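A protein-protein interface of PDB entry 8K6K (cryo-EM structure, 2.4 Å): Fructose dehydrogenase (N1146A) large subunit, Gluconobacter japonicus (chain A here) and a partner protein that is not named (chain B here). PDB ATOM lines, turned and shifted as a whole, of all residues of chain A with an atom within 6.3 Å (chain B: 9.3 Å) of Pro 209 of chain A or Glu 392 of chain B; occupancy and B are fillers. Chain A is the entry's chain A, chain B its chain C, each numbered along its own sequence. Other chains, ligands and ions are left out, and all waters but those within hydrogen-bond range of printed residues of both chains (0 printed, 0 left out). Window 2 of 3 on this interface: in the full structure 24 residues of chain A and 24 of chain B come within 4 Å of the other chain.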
ATOM      1  N   MET A 175      35.104 -25.566  13.214  1.00  0.00           N
ATOM      2  CA  MET A 175      34.080 -24.885  13.988  1.00  0.00           C
ATOM      3  C   MET A 175      33.892 -25.608  15.312  1.00  0.00           C
ATOM      4  O   MET A 175      34.214 -26.789  15.449  1.00  0.00           O
ATOM      5  CB  MET A 175      32.744 -24.819  13.238  1.00  0.00           C
ATOM      6  CG  MET A 175      32.648 -23.700  12.224  1.00  0.00           C
ATOM      7  SD  MET A 175      31.255 -23.900  11.104  1.00  0.00           S
ATOM      8  CE  MET A 175      31.788 -25.317  10.159  1.00  0.00           C
ATOM      9  N   ASN A 206      27.127 -26.139  10.127  1.00  0.00           N
ATOM     10  CA  ASN A 206      27.588 -24.775  10.364  1.00  0.00           C
ATOM     11  C   ASN A 206      27.059 -24.294  11.709  1.00  0.00           C
ATOM     12  O   ASN A 206      25.882 -23.958  11.840  1.00  0.00           O
ATOM     13  CB  ASN A 206      27.141 -23.857   9.234  1.00  0.00           C
ATOM     14  CG  ASN A 206      27.915 -24.087   7.959  1.00  0.00           C
ATOM     15  OD1 ASN A 206      28.922 -24.789   7.951  1.00  0.00           O
ATOM     16  ND2 ASN A 206      27.447 -23.497   6.870  1.00  0.00           N
ATOM     17  N   SER A 207      27.934 -24.260  12.713  1.00  0.00           N
ATOM     18  CA  SER A 207      27.629 -23.546  13.945  1.00  0.00           C
ATOM     19  C   SER A 207      27.828 -22.048  13.791  1.00  0.00           C
ATOM     20  O   SER A 207      27.492 -21.290  14.706  1.00  0.00           O
ATOM     21  CB  SER A 207      28.491 -24.066  15.092  1.00  0.00           C
ATOM     22  OG  SER A 207      29.862 -23.808  14.859  1.00  0.00           O
ATOM     23  N   ARG A 208      28.374 -21.624  12.660  1.00  0.00           N
ATOM     24  CA  ARG A 208      28.513 -20.232  12.269  1.00  0.00           C
ATOM     25  C   ARG A 208      28.581 -20.203  10.753  1.00  0.00           C
ATOM     26  O   ARG A 208      28.841 -21.235  10.126  1.00  0.00           O
ATOM     27  CB  ARG A 208      29.766 -19.599  12.886  1.00  0.00           C
ATOM     28  CG  ARG A 208      31.060 -20.255  12.457  1.00  0.00           C
ATOM     29  CD  ARG A 208      32.261 -19.545  13.044  1.00  0.00           C
ATOM     30  NE  ARG A 208      33.500 -20.261  12.769  1.00  0.00           N
ATOM     31  CZ  ARG A 208      34.146 -20.221  11.612  1.00  0.00           C
ATOM     32  NH1 ARG A 208      33.700 -19.503  10.595  1.00  0.00           N
ATOM     33  NH2 ARG A 208      35.268 -20.918  11.472  1.00  0.00           N
ATOM     34  N   PRO A 209      28.320 -19.056  10.132  1.00  0.00           N
ATOM     35  CA  PRO A 209      28.444 -18.975   8.673  1.00  0.00           C
ATOM     36  C   PRO A 209      29.809 -19.454   8.204  1.00  0.00           C
ATOM     37  O   PRO A 209      30.850 -18.948   8.630  1.00  0.00           O
ATOM     38  CB  PRO A 209      28.234 -17.487   8.390  1.00  0.00           C
ATOM     39  CG  PRO A 209      27.345 -17.043   9.477  1.00  0.00           C
ATOM     40  CD  PRO A 209      27.745 -17.823  10.697  1.00  0.00           C
ATOM     41  N   TYR A 210      29.798 -20.446   7.320  1.00  0.00           N
ATOM     42  CA  TYR A 210      31.011 -21.119   6.886  1.00  0.00           C
ATOM     43  C   TYR A 210      30.876 -21.469   5.415  1.00  0.00           C
ATOM     44  O   TYR A 210      29.817 -21.928   4.979  1.00  0.00           O
ATOM     45  CB  TYR A 210      31.261 -22.383   7.718  1.00  0.00           C
ATOM     46  CG  TYR A 210      32.617 -23.017   7.526  1.00  0.00           C
ATOM     47  CD1 TYR A 210      32.857 -23.881   6.468  1.00  0.00           C
ATOM     48  CD2 TYR A 210      33.652 -22.768   8.414  1.00  0.00           C
ATOM     49  CE1 TYR A 210      34.091 -24.464   6.293  1.00  0.00           C
ATOM     50  CE2 TYR A 210      34.888 -23.351   8.248  1.00  0.00           C
ATOM     51  CZ  TYR A 210      35.101 -24.199   7.187  1.00  0.00           C
ATOM     52  OH  TYR A 210      36.335 -24.781   7.017  1.00  0.00           O
ATOM     53  N   ASP A 211      31.949 -21.244   4.657  1.00  0.00           N
ATOM     54  CA  ASP A 211      32.001 -21.583   3.234  1.00  0.00           C
ATOM     55  C   ASP A 211      30.907 -20.875   2.442  1.00  0.00           C
ATOM     56  O   ASP A 211      30.409 -21.400   1.444  1.00  0.00           O
ATOM     57  CB  ASP A 211      31.919 -23.098   3.028  1.00  0.00           C
ATOM     58  CG  ASP A 211      32.413 -23.532   1.664  1.00  0.00           C
ATOM     59  OD1 ASP A 211      33.260 -22.823   1.083  1.00  0.00           O
ATOM     60  OD2 ASP A 211      31.950 -24.583   1.174  1.00  0.00           O
ATOM     61  N   GLY A 212      30.523 -19.678   2.874  1.00  0.00           N
ATOM     62  CA  GLY A 212      29.456 -18.967   2.202  1.00  0.00           C
ATOM     63  C   GLY A 212      28.089 -19.578   2.380  1.00  0.00           C
ATOM     64  O   GLY A 212      27.183 -19.284   1.597  1.00  0.00           O
ATOM     65  N   ARG A 213      27.910 -20.418   3.393  1.00  0.00           N
ATOM     66  CA  ARG A 213      26.652 -21.090   3.651  1.00  0.00           C
ATOM     67  C   ARG A 213      26.121 -20.692   5.022  1.00  0.00           C
ATOM     68  O   ARG A 213      26.903 -20.374   5.923  1.00  0.00           O
ATOM     69  CB  ARG A 213      26.823 -22.611   3.576  1.00  0.00           C
ATOM     70  CG  ARG A 213      27.201 -23.106   2.194  1.00  0.00           C
ATOM     71  CD  ARG A 213      27.253 -24.614   2.142  1.00  0.00           C
ATOM     72  NE  ARG A 213      28.503 -25.139   2.675  1.00  0.00           N
ATOM     73  CZ  ARG A 213      28.612 -25.789   3.823  1.00  0.00           C
ATOM     74  NH1 ARG A 213      27.561 -26.012   4.593  1.00  0.00           N
ATOM     75  NH2 ARG A 213      29.805 -26.229   4.209  1.00  0.00           N
ATOM     76  N   PRO A 214      24.805 -20.689   5.209  1.00  0.00           N
ATOM     77  CA  PRO A 214      24.237 -20.137   6.441  1.00  0.00           C
ATOM     78  C   PRO A 214      24.524 -21.009   7.652  1.00  0.00           C
ATOM     79  O   PRO A 214      24.833 -22.197   7.551  1.00  0.00           O
ATOM     80  CB  PRO A 214      22.736 -20.088   6.145  1.00  0.00           C
ATOM     81  CG  PRO A 214      22.528 -21.149   5.141  1.00  0.00           C
ATOM     82  CD  PRO A 214      23.758 -21.160   4.288  1.00  0.00           C
ATOM     83  N   GLN A 215      24.429 -20.381   8.819  1.00  0.00           N
ATOM     84  CA  GLN A 215      24.502 -21.105  10.078  1.00  0.00           C
ATOM     85  C   GLN A 215      23.269 -21.983  10.249  1.00  0.00           C
ATOM     86  O   GLN A 215      22.170 -21.639   9.811  1.00  0.00           O
ATOM     87  CB  GLN A 215      24.622 -20.125  11.244  1.00  0.00           C
ATOM     88  CG  GLN A 215      24.805 -20.775  12.598  1.00  0.00           C
ATOM     89  CD  GLN A 215      24.883 -19.764  13.717  1.00  0.00           C
ATOM     90  OE1 GLN A 215      25.114 -18.581  13.482  1.00  0.00           O
ATOM     91  NE2 GLN A 215      24.690 -20.224  14.946  1.00  0.00           N
ATOM     92  N   ARG B  60      38.722 -10.067   3.687  1.00  0.00           N
ATOM     93  CA  ARG B  60      38.846 -10.536   5.063  1.00  0.00           C
ATOM     94  C   ARG B  60      40.174 -11.248   5.281  1.00  0.00           C
ATOM     95  O   ARG B  60      40.746 -11.192   6.376  1.00  0.00           O
ATOM     96  CB  ARG B  60      37.678 -11.458   5.413  1.00  0.00           C
ATOM     97  CG  ARG B  60      36.371 -10.727   5.672  1.00  0.00           C
ATOM     98  CD  ARG B  60      35.494 -11.494   6.649  1.00  0.00           C
ATOM     99  NE  ARG B  60      34.146 -10.944   6.722  1.00  0.00           N
ATOM    100  CZ  ARG B  60      33.093 -11.457   6.102  1.00  0.00           C
ATOM    101  NH1 ARG B  60      33.196 -12.539   5.346  1.00  0.00           N
ATOM    102  NH2 ARG B  60      31.907 -10.874   6.243  1.00  0.00           N
ATOM    103  N   LYS B 257      21.440  -3.846  11.328  1.00  0.00           N
ATOM    104  CA  LYS B 257      20.290  -4.702  11.563  1.00  0.00           C
ATOM    105  C   LYS B 257      19.182  -3.879  12.199  1.00  0.00           C
ATOM    106  O   LYS B 257      19.402  -3.213  13.215  1.00  0.00           O
ATOM    107  CB  LYS B 257      20.662  -5.885  12.460  1.00  0.00           C
ATOM    108  CG  LYS B 257      19.529  -6.854  12.719  1.00  0.00           C
ATOM    109  CD  LYS B 257      20.046  -8.118  13.376  1.00  0.00           C
ATOM    110  CE  LYS B 257      18.914  -8.967  13.913  1.00  0.00           C
ATOM    111  NZ  LYS B 257      19.385 -10.330  14.272  1.00  0.00           N
ATOM    112  N   GLU B 272      30.404  -2.835   8.594  1.00  0.00           N
ATOM    113  CA  GLU B 272      31.247  -3.790   9.295  1.00  0.00           C
ATOM    114  C   GLU B 272      32.718  -3.411   9.293  1.00  0.00           C
ATOM    115  O   GLU B 272      33.484  -3.978  10.078  1.00  0.00           O
ATOM    116  CB  GLU B 272      31.070  -5.184   8.692  1.00  0.00           C
ATOM    117  CG  GLU B 272      32.019  -5.510   7.565  1.00  0.00           C
ATOM    118  CD  GLU B 272      31.844  -6.925   7.061  1.00  0.00           C
ATOM    119  OE1 GLU B 272      30.971  -7.148   6.197  1.00  0.00           O
ATOM    120  OE2 GLU B 272      32.580  -7.818   7.532  1.00  0.00           O
ATOM    121  N   TYR B 358      16.188 -12.735  13.670  1.00  0.00           N
ATOM    122  CA  TYR B 358      17.398 -13.105  12.944  1.00  0.00           C
ATOM    123  C   TYR B 358      17.135 -13.172  11.448  1.00  0.00           C
ATOM    124  O   TYR B 358      17.932 -12.672  10.646  1.00  0.00           O
ATOM    125  CB  TYR B 358      17.938 -14.441  13.453  1.00  0.00           C
ATOM    126  CG  TYR B 358      19.273 -14.822  12.855  1.00  0.00           C
ATOM    127  CD1 TYR B 358      19.346 -15.524  11.663  1.00  0.00           C
ATOM    128  CD2 TYR B 358      20.459 -14.475  13.481  1.00  0.00           C
ATOM    129  CE1 TYR B 358      20.558 -15.867  11.112  1.00  0.00           C
ATOM    130  CE2 TYR B 358      21.678 -14.817  12.936  1.00  0.00           C
ATOM    131  CZ  TYR B 358      21.720 -15.515  11.753  1.00  0.00           C
ATOM    132  OH  TYR B 358      22.931 -15.860  11.205  1.00  0.00           O
ATOM    133  N   TYR B 359      16.023 -13.784  11.053  1.00  0.00           N
ATOM    134  CA  TYR B 359      15.606 -13.784   9.661  1.00  0.00           C
ATOM    135  C   TYR B 359      14.643 -12.627   9.458  1.00  0.00           C
ATOM    136  O   TYR B 359      13.556 -12.630  10.055  1.00  0.00           O
ATOM    137  CB  TYR B 359      14.957 -15.105   9.294  1.00  0.00           C
ATOM    138  CG  TYR B 359      15.909 -16.263   9.437  1.00  0.00           C
ATOM    139  CD1 TYR B 359      17.157 -16.223   8.840  1.00  0.00           C
ATOM    140  CD2 TYR B 359      15.578 -17.380  10.187  1.00  0.00           C
ATOM    141  CE1 TYR B 359      18.040 -17.262   8.970  1.00  0.00           C
ATOM    142  CE2 TYR B 359      16.460 -18.430  10.321  1.00  0.00           C
ATOM    143  CZ  TYR B 359      17.690 -18.361   9.709  1.00  0.00           C
ATOM    144  OH  TYR B 359      18.586 -19.392   9.828  1.00  0.00           O
ATOM    145  N   VAL B 384      23.386 -11.974   1.716  1.00  0.00           N
ATOM    146  CA  VAL B 384      23.799 -10.964   2.678  1.00  0.00           C
ATOM    147  C   VAL B 384      24.907 -11.555   3.535  1.00  0.00           C
ATOM    148  O   VAL B 384      24.807 -12.699   3.989  1.00  0.00           O
ATOM    149  CB  VAL B 384      22.622 -10.499   3.560  1.00  0.00           C
ATOM    150  CG1 VAL B 384      23.038  -9.321   4.415  1.00  0.00           C
ATOM    151  CG2 VAL B 384      21.422 -10.149   2.703  1.00  0.00           C
ATOM    152  N   ASP B 385      25.966 -10.780   3.745  1.00  0.00           N
ATOM    153  CA  ASP B 385      27.077 -11.221   4.583  1.00  0.00           C
ATOM    154  C   ASP B 385      27.588 -10.013   5.350  1.00  0.00           C
ATOM    155  O   ASP B 385      28.295  -9.175   4.785  1.00  0.00           O
ATOM    156  CB  ASP B 385      28.184 -11.852   3.745  1.00  0.00           C
ATOM    157  CG  ASP B 385      29.121 -12.704   4.569  1.00  0.00           C
ATOM    158  OD1 ASP B 385      28.981 -12.710   5.807  1.00  0.00           O
ATOM    159  OD2 ASP B 385      29.998 -13.369   3.982  1.00  0.00           O
ATOM    160  N   ARG B 386      27.233  -9.924   6.629  1.00  0.00           N
ATOM    161  CA  ARG B 386      27.608  -8.790   7.462  1.00  0.00           C
ATOM    162  C   ARG B 386      28.128  -9.311   8.791  1.00  0.00           C
ATOM    163  O   ARG B 386      27.425 -10.047   9.486  1.00  0.00           O
ATOM    164  CB  ARG B 386      26.417  -7.855   7.676  1.00  0.00           C
ATOM    165  CG  ARG B 386      26.765  -6.507   8.271  1.00  0.00           C
ATOM    166  CD  ARG B 386      25.544  -5.875   8.906  1.00  0.00           C
ATOM    167  NE  ARG B 386      24.314  -6.386   8.316  1.00  0.00           N
ATOM    168  CZ  ARG B 386      23.367  -7.025   8.990  1.00  0.00           C
ATOM    169  NH1 ARG B 386      23.469  -7.239  10.290  1.00  0.00           N
ATOM    170  NH2 ARG B 386      22.294  -7.464   8.342  1.00  0.00           N
ATOM    171  N   THR B 387      29.353  -8.928   9.139  1.00  0.00           N
ATOM    172  CA  THR B 387      29.990  -9.335  10.387  1.00  0.00           C
ATOM    173  C   THR B 387      30.121  -8.112  11.283  1.00  0.00           C
ATOM    174  O   THR B 387      30.999  -7.272  11.071  1.00  0.00           O
ATOM    175  CB  THR B 387      31.356  -9.964  10.128  1.00  0.00           C
ATOM    176  OG1 THR B 387      31.266 -10.867   9.020  1.00  0.00           O
ATOM    177  CG2 THR B 387      31.833 -10.719  11.353  1.00  0.00           C
ATOM    178  N   THR B 388      29.255  -8.018  12.285  1.00  0.00           N
ATOM    179  CA  THR B 388      29.284  -6.934  13.254  1.00  0.00           C
ATOM    180  C   THR B 388      29.521  -7.521  14.636  1.00  0.00           C
ATOM    181  O   THR B 388      28.847  -8.479  15.026  1.00  0.00           O
ATOM    182  CB  THR B 388      27.980  -6.131  13.221  1.00  0.00           C
ATOM    183  OG1 THR B 388      27.987  -5.258  12.086  1.00  0.00           O
ATOM    184  CG2 THR B 388      27.822  -5.304  14.483  1.00  0.00           C
ATOM    185  N   ASP B 389      30.482  -6.950  15.363  1.00  0.00           N
ATOM    186  CA  ASP B 389      30.840  -7.412  16.705  1.00  0.00           C
ATOM    187  C   ASP B 389      31.279  -8.874  16.693  1.00  0.00           C
ATOM    188  O   ASP B 389      30.949  -9.648  17.593  1.00  0.00           O
ATOM    189  CB  ASP B 389      29.687  -7.199  17.689  1.00  0.00           C
ATOM    190  CG  ASP B 389      30.131  -6.524  18.967  1.00  0.00           C
ATOM    191  OD1 ASP B 389      31.163  -6.939  19.532  1.00  0.00           O
ATOM    192  OD2 ASP B 389      29.447  -5.575  19.405  1.00  0.00           O
ATOM    193  N   ASN B 390      32.022  -9.255  15.652  1.00  0.00           N
ATOM    194  CA  ASN B 390      32.576 -10.598  15.483  1.00  0.00           C
ATOM    195  C   ASN B 390      31.497 -11.668  15.354  1.00  0.00           C
ATOM    196  O   ASN B 390      31.787 -12.861  15.476  1.00  0.00           O
ATOM    197  CB  ASN B 390      33.537 -10.951  16.623  1.00  0.00           C
ATOM    198  CG  ASN B 390      34.807 -10.131  16.587  1.00  0.00           C
ATOM    199  OD1 ASN B 390      35.100  -9.377  17.514  1.00  0.00           O
ATOM    200  ND2 ASN B 390      35.572 -10.272  15.511  1.00  0.00           N
ATOM    201  N   HIS B 391      30.255 -11.267  15.105  1.00  0.00           N
ATOM    202  CA  HIS B 391      29.157 -12.187  14.847  1.00  0.00           C
ATOM    203  C   HIS B 391      28.701 -11.990  13.411  1.00  0.00           C
ATOM    204  O   HIS B 391      28.464 -10.856  12.985  1.00  0.00           O
ATOM    205  CB  HIS B 391      27.997 -11.956  15.818  1.00  0.00           C
ATOM    206  CG  HIS B 391      26.816 -12.839  15.566  1.00  0.00           C
ATOM    207  ND1 HIS B 391      26.886 -14.214  15.637  1.00  0.00           N
ATOM    208  CD2 HIS B 391      25.536 -12.545  15.240  1.00  0.00           C
ATOM    209  CE1 HIS B 391      25.700 -14.728  15.366  1.00  0.00           C
ATOM    210  NE2 HIS B 391      24.863 -13.736  15.123  1.00  0.00           N
ATOM    211  N   GLU B 392      28.576 -13.085  12.669  1.00  0.00           N
ATOM    212  CA  GLU B 392      28.362 -13.025  11.229  1.00  0.00           C
ATOM    213  C   GLU B 392      26.929 -13.398  10.876  1.00  0.00           C
ATOM    214  O   GLU B 392      26.476 -14.508  11.172  1.00  0.00           O
ATOM    215  CB  GLU B 392      29.343 -13.941  10.499  1.00  0.00           C
ATOM    216  CG  GLU B 392      29.543 -13.579   9.040  1.00  0.00           C
ATOM    217  CD  GLU B 392      30.356 -14.609   8.290  1.00  0.00           C
ATOM    218  OE1 GLU B 392      31.351 -15.110   8.852  1.00  0.00           O
ATOM    219  OE2 GLU B 392      30.008 -14.912   7.133  1.00  0.00           O
ATOM    220  N   ILE B 393      26.217 -12.452  10.266  1.00  0.00           N
ATOM    221  CA  ILE B 393      25.070 -12.762   9.426  1.00  0.00           C
ATOM    222  C   ILE B 393      25.517 -13.494   8.170  1.00  0.00           C
ATOM    223  O   ILE B 393      26.627 -13.285   7.662  1.00  0.00           O
ATOM    224  CB  ILE B 393      24.321 -11.464   9.064  1.00  0.00           C
ATOM    225  CG1 ILE B 393      23.112 -11.214   9.982  1.00  0.00           C
ATOM    226  CG2 ILE B 393      24.099 -11.351   7.556  1.00  0.00           C
ATOM    227  CD1 ILE B 393      23.459 -11.198  11.456  1.00  0.00           C
ATOM    228  N   LEU B 394      24.649 -14.364   7.655  1.00  0.00           N
ATOM    229  CA  LEU B 394      24.838 -14.854   6.299  1.00  0.00           C
ATOM    230  C   LEU B 394      23.513 -15.292   5.695  1.00  0.00           C
ATOM    231  O   LEU B 394      22.808 -16.130   6.262  1.00  0.00           O
ATOM    232  CB  LEU B 394      25.838 -16.010   6.243  1.00  0.00           C
ATOM    233  CG  LEU B 394      26.416 -16.217   4.842  1.00  0.00           C
ATOM    234  CD1 LEU B 394      27.920 -16.373   4.903  1.00  0.00           C
ATOM    235  CD2 LEU B 394      25.780 -17.405   4.148  1.00  0.00           C
ATOM    236  N   MET B 395      23.187 -14.694   4.553  1.00  0.00           N
ATOM    237  CA  MET B 395      22.252 -15.228   3.578  1.00  0.00           C
ATOM    238  C   MET B 395      23.026 -15.994   2.521  1.00  0.00           C
ATOM    239  O   MET B 395      23.975 -15.441   1.945  1.00  0.00           O
ATOM    240  CB  MET B 395      21.459 -14.112   2.917  1.00  0.00           C
ATOM    241  CG  MET B 395      20.197 -14.560   2.234  1.00  0.00           C
ATOM    242  SD  MET B 395      19.384 -13.151   1.482  1.00  0.00           S
ATOM    243  CE  MET B 395      18.631 -13.948   0.071  1.00  0.00           C
ATOM    244  N   PRO B 396      22.680 -17.244   2.231  1.00  0.00           N
ATOM    245  CA  PRO B 396      23.307 -17.926   1.097  1.00  0.00           C
ATOM    246  C   PRO B 396      22.962 -17.228  -0.210  1.00  0.00           C
ATOM    247  O   PRO B 396      21.869 -16.686  -0.377  1.00  0.00           O
ATOM    248  CB  PRO B 396      22.713 -19.336   1.162  1.00  0.00           C
ATOM    249  CG  PRO B 396      21.423 -19.164   1.880  1.00  0.00           C
ATOM    250  CD  PRO B 396      21.644 -18.067   2.873  1.00  0.00           C
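The side-chain amide nitrogen of Asn 206 of chain A sits at hydrogen-bond distance from the backbone carbonyl oxygen of Pro 214 of chain A, 3.0 Å away.
OD2 of Asp 211 of chain A lies within salt-bridge range of NE of Arg 213 of chain A (3.8 Å).
The side-chain amide nitrogen (ND2) of Asn 206 of chain A lies within hydrogen-bond range of the backbone carbonyl oxygen (O) of Arg 213 of chain A.
Among the printed residues, merely in contact across the chains: Pro 209 of chain A with Glu 392 of chain B (3.2 Å), Arg 213 of chain A with Leu 394 of chain B (3.4 Å), Gly 212 of chain A with Leu 394 of chain B (3.5 Å), Pro 209 of chain A with Leu 394 of chain B (3.5 Å), Pro 214 of chain A with Leu 394 of chain B (3.6 Å) and Pro 214 of chain A with Pro 396 of chain B (3.8 Å).
Arg 208 of chain A touches none of the printed residues of chain B.
Of the printed residues of chain B, Pro 209 of chain A touches Glu 392 (3.2 Å) and Leu 394 (3.5 Å).
Of the printed residues of chain B, Gly 212 of chain A touches Leu 394.
Printed residues of chain B within 4 Å of Arg 213 of chain A: Leu 394 (3.4 Å).
Asp 385 of chain B touches none of the printed residues of chain A.
Glu 392 of chain B touches just one residue of chain A: Pro 209.
Of the printed residues of chain A, Leu 394 of chain B touches Pro 209 (3.5 Å), Gly 212 (3.5 Å), Arg 213 (3.4 Å) and Pro 214 (3.6 Å).
Of the printed residues of chain A, Pro 396 of chain B touches Pro 214.
The nearest residue of chain B that does not touch Pro 209 of chain A is Ile 393 of chain B (4.2 Å).
The nearest printed residue of chain B that does not touch Arg 213 of chain A is Pro 396 of chain B (5.0 Å).
Along chain A the printed residues that touch a printed residue of chain B span positions 209 to 214.
Of the 18 printed residues of chain B, 3 touch a printed residue of chain A.
Printed residues of chain B that touch a printed residue of chain A: Glu 392, Leu 394 and Pro 396.
Hydrophobic or aromatic side chains of chain B that line the printed part of chain A: Leu 394 and Pro 396.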
